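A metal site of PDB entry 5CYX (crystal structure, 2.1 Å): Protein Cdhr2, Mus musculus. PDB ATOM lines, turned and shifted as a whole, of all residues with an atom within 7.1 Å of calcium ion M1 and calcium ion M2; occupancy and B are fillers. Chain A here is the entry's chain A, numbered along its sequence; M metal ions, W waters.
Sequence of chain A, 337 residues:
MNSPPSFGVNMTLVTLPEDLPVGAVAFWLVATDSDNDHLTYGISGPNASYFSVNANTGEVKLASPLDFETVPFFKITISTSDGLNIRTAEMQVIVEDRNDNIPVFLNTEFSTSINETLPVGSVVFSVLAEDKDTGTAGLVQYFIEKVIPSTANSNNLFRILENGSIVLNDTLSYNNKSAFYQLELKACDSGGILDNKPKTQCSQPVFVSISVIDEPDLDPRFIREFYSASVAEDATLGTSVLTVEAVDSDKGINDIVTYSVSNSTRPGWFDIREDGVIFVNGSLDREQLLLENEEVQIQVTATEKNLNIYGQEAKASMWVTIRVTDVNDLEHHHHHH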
ATOM      1  N   GLU A 116      20.521  24.512 -18.960  1.00  0.00           N
ATOM      2  CA  GLU A 116      20.080  23.184 -18.503  1.00  0.00           C
ATOM      3  C   GLU A 116      20.823  22.779 -17.213  1.00  0.00           C
ATOM      4  O   GLU A 116      20.272  21.978 -16.478  1.00  0.00           O
ATOM      5  CB  GLU A 116      20.222  22.104 -19.557  1.00  0.00           C
ATOM      6  CG  GLU A 116      21.619  21.564 -19.816  1.00  0.00           C
ATOM      7  CD  GLU A 116      21.725  20.609 -21.015  1.00  0.00           C
ATOM      8  OE1 GLU A 116      20.785  19.798 -21.355  1.00  0.00           O
ATOM      9  OE2 GLU A 116      22.842  20.621 -21.595  1.00  0.00           O
ATOM     10  N   SER A 173      17.199  18.694 -18.895  1.00  0.00           N
ATOM     11  CA  SER A 173      18.044  18.193 -20.002  1.00  0.00           C
ATOM     12  C   SER A 173      17.456  18.574 -21.353  1.00  0.00           C
ATOM     13  O   SER A 173      16.398  18.052 -21.729  1.00  0.00           O
ATOM     14  CB  SER A 173      18.208  16.661 -19.961  1.00  0.00           C
ATOM     15  OG  SER A 173      19.039  16.245 -21.065  1.00  0.00           O
ATOM     16  N   TYR A 174      18.135  19.475 -22.065  1.00  0.00           N
ATOM     17  CA  TYR A 174      17.745  19.854 -23.413  1.00  0.00           C
ATOM     18  C   TYR A 174      17.534  18.632 -24.318  1.00  0.00           C
ATOM     19  O   TYR A 174      16.571  18.567 -25.025  1.00  0.00           O
ATOM     20  CB  TYR A 174      18.778  20.832 -24.040  1.00  0.00           C
ATOM     21  CG  TYR A 174      18.516  21.201 -25.497  1.00  0.00           C
ATOM     22  CD1 TYR A 174      18.840  20.346 -26.536  1.00  0.00           C
ATOM     23  CD2 TYR A 174      17.975  22.448 -25.849  1.00  0.00           C
ATOM     24  CE1 TYR A 174      18.599  20.706 -27.886  1.00  0.00           C
ATOM     25  CE2 TYR A 174      17.708  22.790 -27.180  1.00  0.00           C
ATOM     26  CZ  TYR A 174      18.043  21.931 -28.190  1.00  0.00           C
ATOM     27  OH  TYR A 174      17.811  22.279 -29.531  1.00  0.00           O
ATOM     28  N   ASN A 175      18.459  17.700 -24.308  1.00  0.00           N
ATOM     29  CA  ASN A 175      18.472  16.515 -25.174  1.00  0.00           C
ATOM     30  C   ASN A 175      17.688  15.285 -24.666  1.00  0.00           C
ATOM     31  O   ASN A 175      17.202  14.516 -25.453  1.00  0.00           O
ATOM     32  CB  ASN A 175      19.929  16.103 -25.375  1.00  0.00           C
ATOM     33  CG  ASN A 175      20.698  17.166 -26.111  1.00  0.00           C
ATOM     34  OD1 ASN A 175      21.430  18.007 -25.516  1.00  0.00           O
ATOM     35  ND2 ASN A 175      20.469  17.211 -27.382  1.00  0.00           N
ATOM     36  N   ILE A 213      18.443  25.960 -22.541  1.00  0.00           N
ATOM     37  CA  ILE A 213      19.652  26.162 -23.329  1.00  0.00           C
ATOM     38  C   ILE A 213      20.557  24.956 -23.171  1.00  0.00           C
ATOM     39  O   ILE A 213      20.882  24.511 -22.042  1.00  0.00           O
ATOM     40  CB  ILE A 213      20.399  27.418 -22.847  1.00  0.00           C
ATOM     41  CG1 ILE A 213      19.578  28.673 -23.145  1.00  0.00           C
ATOM     42  CG2 ILE A 213      21.819  27.528 -23.422  1.00  0.00           C
ATOM     43  CD1 ILE A 213      20.099  29.909 -22.411  1.00  0.00           C
ATOM     44  N   ASP A 214      20.954  24.401 -24.301  1.00  0.00           N
ATOM     45  CA  ASP A 214      21.787  23.225 -24.331  1.00  0.00           C
ATOM     46  C   ASP A 214      23.221  23.654 -23.992  1.00  0.00           C
ATOM     47  O   ASP A 214      23.762  24.636 -24.568  1.00  0.00           O
ATOM     48  CB  ASP A 214      21.735  22.546 -25.691  1.00  0.00           C
ATOM     49  CG  ASP A 214      22.240  21.111 -25.668  1.00  0.00           C
ATOM     50  OD1 ASP A 214      22.640  20.566 -24.551  1.00  0.00           O
ATOM     51  OD2 ASP A 214      22.222  20.538 -26.764  1.00  0.00           O
ATOM     52  N   GLU A 215      23.809  22.933 -23.030  1.00  0.00           N
ATOM     53  CA  GLU A 215      25.190  23.190 -22.627  1.00  0.00           C
ATOM     54  C   GLU A 215      26.064  21.975 -22.943  1.00  0.00           C
ATOM     55  O   GLU A 215      25.547  20.894 -23.040  1.00  0.00           O
ATOM     56  CB  GLU A 215      25.265  23.521 -21.153  1.00  0.00           C
ATOM     57  CG  GLU A 215      24.636  24.864 -20.782  1.00  0.00           C
ATOM     58  CD  GLU A 215      24.777  25.113 -19.282  1.00  0.00           C
ATOM     59  OE1 GLU A 215      23.999  24.589 -18.459  1.00  0.00           O
ATOM     60  OE2 GLU A 215      25.723  25.820 -18.914  1.00  0.00           O
ATOM     61  N   PRO A 216      27.367  22.185 -23.176  1.00  0.00           N
ATOM     62  CA  PRO A 216      28.169  21.082 -23.671  1.00  0.00           C
ATOM     63  C   PRO A 216      28.576  20.117 -22.546  1.00  0.00           C
ATOM     64  O   PRO A 216      29.570  20.353 -21.867  1.00  0.00           O
ATOM     65  CB  PRO A 216      29.366  21.766 -24.289  1.00  0.00           C
ATOM     66  CG  PRO A 216      29.485  23.071 -23.570  1.00  0.00           C
ATOM     67  CD  PRO A 216      28.089  23.473 -23.202  1.00  0.00           C
ATOM     68  N   ASP A 217      27.759  19.085 -22.339  1.00  0.00           N
ATOM     69  CA  ASP A 217      28.047  18.077 -21.312  1.00  0.00           C
ATOM     70  C   ASP A 217      27.728  16.653 -21.715  1.00  0.00           C
ATOM     71  O   ASP A 217      27.596  15.810 -20.852  1.00  0.00           O
ATOM     72  CB  ASP A 217      27.256  18.422 -20.041  1.00  0.00           C
ATOM     73  CG  ASP A 217      25.738  18.374 -20.243  1.00  0.00           C
ATOM     74  OD1 ASP A 217      25.200  18.264 -21.386  1.00  0.00           O
ATOM     75  OD2 ASP A 217      25.072  18.461 -19.217  1.00  0.00           O
ATOM     76  N   LEU A 218      27.597  16.404 -23.009  1.00  0.00           N
ATOM     77  CA  LEU A 218      27.433  15.063 -23.519  1.00  0.00           C
ATOM     78  C   LEU A 218      28.544  14.839 -24.518  1.00  0.00           C
ATOM     79  O   LEU A 218      28.850  15.725 -25.373  1.00  0.00           O
ATOM     80  CB  LEU A 218      26.055  14.925 -24.158  1.00  0.00           C
ATOM     81  CG  LEU A 218      24.869  15.030 -23.210  1.00  0.00           C
ATOM     82  CD1 LEU A 218      23.580  15.080 -24.008  1.00  0.00           C
ATOM     83  CD2 LEU A 218      24.839  13.831 -22.266  1.00  0.00           C
ATOM     84  N   ASP A 219      29.159  13.663 -24.433  1.00  0.00           N
ATOM     85  CA  ASP A 219      30.256  13.319 -25.318  1.00  0.00           C
ATOM     86  C   ASP A 219      29.744  13.043 -26.737  1.00  0.00           C
ATOM     87  O   ASP A 219      28.562  12.788 -26.928  1.00  0.00           O
ATOM     88  CB  ASP A 219      31.040  12.098 -24.771  1.00  0.00           C
ATOM     89  CG  ASP A 219      31.930  12.443 -23.549  1.00  0.00           C
ATOM     90  OD1 ASP A 219      32.216  13.638 -23.293  1.00  0.00           O
ATOM     91  OD2 ASP A 219      32.362  11.496 -22.864  1.00  0.00           O
ATOM     92  N   PRO A 220      30.637  13.108 -27.749  1.00  0.00           N
ATOM     93  CA  PRO A 220      30.289  12.712 -29.122  1.00  0.00           C
ATOM     94  C   PRO A 220      30.097  11.218 -29.304  1.00  0.00           C
ATOM     95  O   PRO A 220      30.703  10.441 -28.577  1.00  0.00           O
ATOM     96  CB  PRO A 220      31.507  13.158 -29.916  1.00  0.00           C
ATOM     97  CG  PRO A 220      32.620  13.048 -28.945  1.00  0.00           C
ATOM     98  CD  PRO A 220      32.050  13.519 -27.640  1.00  0.00           C
ATOM     99  N   VAL A 247      29.465  12.441 -34.008  1.00  0.00           N
ATOM    100  CA  VAL A 247      28.779  13.723 -33.897  1.00  0.00           C
ATOM    101  C   VAL A 247      28.485  14.053 -32.443  1.00  0.00           C
ATOM    102  O   VAL A 247      28.313  13.158 -31.605  1.00  0.00           O
ATOM    103  CB  VAL A 247      27.459  13.777 -34.713  1.00  0.00           C
ATOM    104  CG1 VAL A 247      27.746  13.505 -36.198  1.00  0.00           C
ATOM    105  CG2 VAL A 247      26.447  12.779 -34.200  1.00  0.00           C
ATOM    106  N   ASP A 248      28.395  15.342 -32.174  1.00  0.00           N
ATOM    107  CA  ASP A 248      28.137  15.869 -30.850  1.00  0.00           C
ATOM    108  C   ASP A 248      26.720  15.477 -30.409  1.00  0.00           C
ATOM    109  O   ASP A 248      25.761  15.738 -31.123  1.00  0.00           O
ATOM    110  CB  ASP A 248      28.307  17.382 -30.893  1.00  0.00           C
ATOM    111  CG  ASP A 248      28.092  18.046 -29.585  1.00  0.00           C
ATOM    112  OD1 ASP A 248      27.973  17.340 -28.569  1.00  0.00           O
ATOM    113  OD2 ASP A 248      28.071  19.298 -29.573  1.00  0.00           O
ATOM    114  N   SER A 249      26.619  14.842 -29.229  1.00  0.00           N
ATOM    115  CA  SER A 249      25.315  14.460 -28.692  1.00  0.00           C
ATOM    116  C   SER A 249      24.526  15.643 -28.184  1.00  0.00           C
ATOM    117  O   SER A 249      23.317  15.544 -28.015  1.00  0.00           O
ATOM    118  CB  SER A 249      25.471  13.394 -27.588  1.00  0.00           C
ATOM    119  OG  SER A 249      26.138  12.295 -28.111  1.00  0.00           O
ATOM    120  N   ASP A 250      25.189  16.791 -27.962  1.00  0.00           N
ATOM    121  CA  ASP A 250      24.481  17.999 -27.600  1.00  0.00           C
ATOM    122  C   ASP A 250      23.933  18.613 -28.903  1.00  0.00           C
ATOM    123  O   ASP A 250      24.619  19.396 -29.619  1.00  0.00           O
ATOM    124  CB  ASP A 250      25.380  18.990 -26.826  1.00  0.00           C
ATOM    125  CG  ASP A 250      26.025  18.375 -25.579  1.00  0.00           C
ATOM    126  OD1 ASP A 250      25.353  18.219 -24.596  1.00  0.00           O
ATOM    127  OD2 ASP A 250      27.233  18.033 -25.603  1.00  0.00           O
ATOM    128  N   LYS A 251      22.671  18.307 -29.179  1.00  0.00           N
ATOM    129  CA  LYS A 251      22.027  18.644 -30.466  1.00  0.00           C
ATOM    130  C   LYS A 251      21.661  20.132 -30.569  1.00  0.00           C
ATOM    131  O   LYS A 251      21.384  20.586 -31.634  1.00  0.00           O
ATOM    132  CB  LYS A 251      20.787  17.781 -30.750  1.00  0.00           C
ATOM    133  CG  LYS A 251      21.010  16.285 -30.680  1.00  0.00           C
ATOM    134  CD  LYS A 251      21.959  15.776 -31.740  1.00  0.00           C
ATOM    135  CE  LYS A 251      22.149  14.267 -31.590  1.00  0.00           C
ATOM    136  NZ  LYS A 251      23.342  13.790 -32.328  1.00  0.00           N
ATOM    137  N   GLY A 252      21.635  20.840 -29.461  1.00  0.00           N
ATOM    138  CA  GLY A 252      21.509  22.280 -29.471  1.00  0.00           C
ATOM    139  C   GLY A 252      22.810  23.019 -29.749  1.00  0.00           C
ATOM    140  O   GLY A 252      22.808  24.227 -29.856  1.00  0.00           O
ATOM    141  N   ILE A 253      23.900  22.279 -29.849  1.00  0.00           N
ATOM    142  CA  ILE A 253      25.225  22.783 -30.012  1.00  0.00           C
ATOM    143  C   ILE A 253      25.820  22.291 -31.316  1.00  0.00           C
ATOM    144  O   ILE A 253      26.250  23.115 -32.102  1.00  0.00           O
ATOM    145  CB  ILE A 253      26.137  22.479 -28.770  1.00  0.00           C
ATOM    146  CG1 ILE A 253      25.640  23.274 -27.559  1.00  0.00           C
ATOM    147  CG2 ILE A 253      27.590  22.919 -29.007  1.00  0.00           C
ATOM    148  CD1 ILE A 253      26.126  22.779 -26.185  1.00  0.00           C
ATOM    149  N   ASN A 254      25.831  20.994 -31.561  1.00  0.00           N
ATOM    150  CA  ASN A 254      26.523  20.384 -32.734  1.00  0.00           C
ATOM    151  C   ASN A 254      27.898  21.022 -32.999  1.00  0.00           C
ATOM    152  O   ASN A 254      28.139  21.608 -34.062  1.00  0.00           O
ATOM    153  CB  ASN A 254      25.698  20.413 -34.043  1.00  0.00           C
ATOM    154  CG  ASN A 254      24.221  20.342 -33.818  1.00  0.00           C
ATOM    155  OD1 ASN A 254      23.684  19.274 -33.449  1.00  0.00           O
ATOM    156  ND2 ASN A 254      23.520  21.452 -34.086  1.00  0.00           N
ATOM    157  N   ASP A 255      28.765  20.872 -32.007  1.00  0.00           N
ATOM    158  CA  ASP A 255      30.158  21.307 -31.997  1.00  0.00           C
ATOM    159  C   ASP A 255      30.872  20.484 -33.059  1.00  0.00           C
ATOM    160  O   ASP A 255      30.548  19.311 -33.239  1.00  0.00           O
ATOM    161  CB  ASP A 255      30.779  20.998 -30.608  1.00  0.00           C
ATOM    162  CG  ASP A 255      32.094  21.746 -30.345  1.00  0.00           C
ATOM    163  OD1 ASP A 255      32.594  22.492 -31.203  1.00  0.00           O
ATOM    164  OD2 ASP A 255      32.651  21.561 -29.236  1.00  0.00           O
ATOM    165  N   GLU A 304      35.617  16.701 -29.476  1.00  0.00           N
ATOM    166  CA  GLU A 304      34.949  17.945 -29.778  1.00  0.00           C
ATOM    167  C   GLU A 304      35.965  19.062 -29.742  1.00  0.00           C
ATOM    168  O   GLU A 304      36.983  18.967 -29.070  1.00  0.00           O
ATOM    169  CB  GLU A 304      33.790  18.212 -28.830  1.00  0.00           C
ATOM    170  CG  GLU A 304      32.657  17.213 -29.044  1.00  0.00           C
ATOM    171  CD  GLU A 304      31.488  17.333 -28.074  1.00  0.00           C
ATOM    172  OE1 GLU A 304      31.316  18.373 -27.427  1.00  0.00           O
ATOM    173  OE2 GLU A 304      30.673  16.410 -28.018  1.00  0.00           O
ATOM    174  N   ASN A 306      35.580  22.248 -28.701  1.00  0.00           N
ATOM    175  CA  ASN A 306      35.497  23.001 -27.476  1.00  0.00           C
ATOM    176  C   ASN A 306      35.417  22.087 -26.265  1.00  0.00           C
ATOM    177  O   ASN A 306      34.934  20.943 -26.347  1.00  0.00           O
ATOM    178  CB  ASN A 306      34.282  23.923 -27.515  1.00  0.00           C
ATOM    179  CG  ASN A 306      34.381  24.925 -28.659  1.00  0.00           C
ATOM    180  OD1 ASN A 306      33.855  24.706 -29.753  1.00  0.00           O
ATOM    181  ND2 ASN A 306      35.137  25.972 -28.435  1.00  0.00           N
ATOM    182  N   ASN A 308      34.182  20.815 -22.580  1.00  0.00           N
ATOM    183  CA  ASN A 308      32.883  20.704 -21.958  1.00  0.00           C
ATOM    184  C   ASN A 308      32.742  21.693 -20.792  1.00  0.00           C
ATOM    185  O   ASN A 308      33.680  22.421 -20.493  1.00  0.00           O
ATOM    186  CB  ASN A 308      32.576  19.232 -21.597  1.00  0.00           C
ATOM    187  CG  ASN A 308      33.434  18.661 -20.446  1.00  0.00           C
ATOM    188  OD1 ASN A 308      34.057  19.375 -19.646  1.00  0.00           O
ATOM    189  ND2 ASN A 308      33.429  17.359 -20.352  1.00  0.00           N
ATOM    190  N   ILE A 309      31.569  21.727 -20.177  1.00  0.00           N
ATOM    191  CA  ILE A 309      31.300  22.616 -19.035  1.00  0.00           C
ATOM    192  C   ILE A 309      32.267  22.462 -17.853  1.00  0.00           C
ATOM    193  O   ILE A 309      32.428  23.397 -17.086  1.00  0.00           O
ATOM    194  CB  ILE A 309      29.857  22.460 -18.483  1.00  0.00           C
ATOM    195  CG1 ILE A 309      29.559  21.027 -18.018  1.00  0.00           C
ATOM    196  CG2 ILE A 309      28.843  22.896 -19.517  1.00  0.00           C
ATOM    197  CD1 ILE A 309      28.251  20.933 -17.277  1.00  0.00           C
ATOM    198  N   ALA A 314      35.752  16.419 -24.516  1.00  0.00           N
ATOM    199  CA  ALA A 314      34.598  15.588 -24.786  1.00  0.00           C
ATOM    200  C   ALA A 314      35.031  14.707 -25.932  1.00  0.00           C
ATOM    201  O   ALA A 314      35.226  15.195 -27.055  1.00  0.00           O
ATOM    202  CB  ALA A 314      33.411  16.451 -25.170  1.00  0.00           C
HETATM  203 CA    CA M   1      29.203  17.705 -26.517  1.00  0.00          CA
HETATM  204 CA    CA M   2      23.924  19.287 -23.086  1.00  0.00          CA
HETATM  205  O   HOH W   1      28.938  20.094 -27.171  1.00  0.00           O
HETATM  206  O   HOH W   2      30.513  18.279 -24.411  1.00  0.00           O
HETATM  207  O   HOH W   3      21.990  17.950 -22.770  1.00  0.00           O
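Calcium ion M2 is bound by OE2 of Glu 116 (2.3 Å), O of Glu 215 (2.3 Å), OD1 of Asp 214 (2.3 Å), OD1 of Asp 250 (2.3 Å), OD1 of Asp 217 (2.4 Å) and water W3 (2.4 Å).
Calcium ion M2 has six donor atoms within binding distance.
The side-chain carboxylate (OE1) of Glu 116 is in hydrogen-bond range of the backbone NH (N) of Tyr 174.
The backbone NH (N) of Glu 116 lies within hydrogen-bond range of the backbone carbonyl oxygen (O) of Ile 213 (3.1 Å).
N of Glu 304 sits at hydrogen-bond distance from O of Ala 314, at 2.9 Å.
The side-chain carboxylate (OD2) of Asp 248 lies within hydrogen-bond range of the backbone NH (N) of Asp 255 (3.0 Å).
O of Asp 248 sits at hydrogen-bond distance from NZ of Lys 251, at 3.3 Å.
The side-chain carboxylate of Asp 248 sits at hydrogen-bond distance from the backbone NH of Asn 254 (3.4 Å).
The side-chain amide nitrogen (ND2) of Asn 175 sits at hydrogen-bond distance from the backbone carbonyl oxygen (O) of Ser 249.
The side-chain amide nitrogen (ND2) of Asn 175 lies close to the backbone NH (N) of Lys 251 (3.0 Å).
Calcium ion M1 is bound by the side-chain carboxylate (OD2) of Asp 250, the backbone carbonyl oxygen (O) of Leu 218, the side-chain carboxylate (OE1) of Glu 304, the side-chain carboxylate (OD1) of Asp 248, the side-chain carboxylate (OE2) of Glu 304, water W1 and water W2.
Calcium ion M1 has seven donor atoms within binding distance.
OD1 of Asn 175 touches calcium ion M2 (3.7 Å).
Six residues have an atom within 4 Å of calcium ion M2: Glu 116, Asn 175, Asp 214, Glu 215, Asp 217 and Asp 250.
Along chain A the residues within 4 Å of calcium ion M2 span positions 116 to 250.
Water W3 bridges OE1 of Glu 116 and OD1 of Asn 175.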
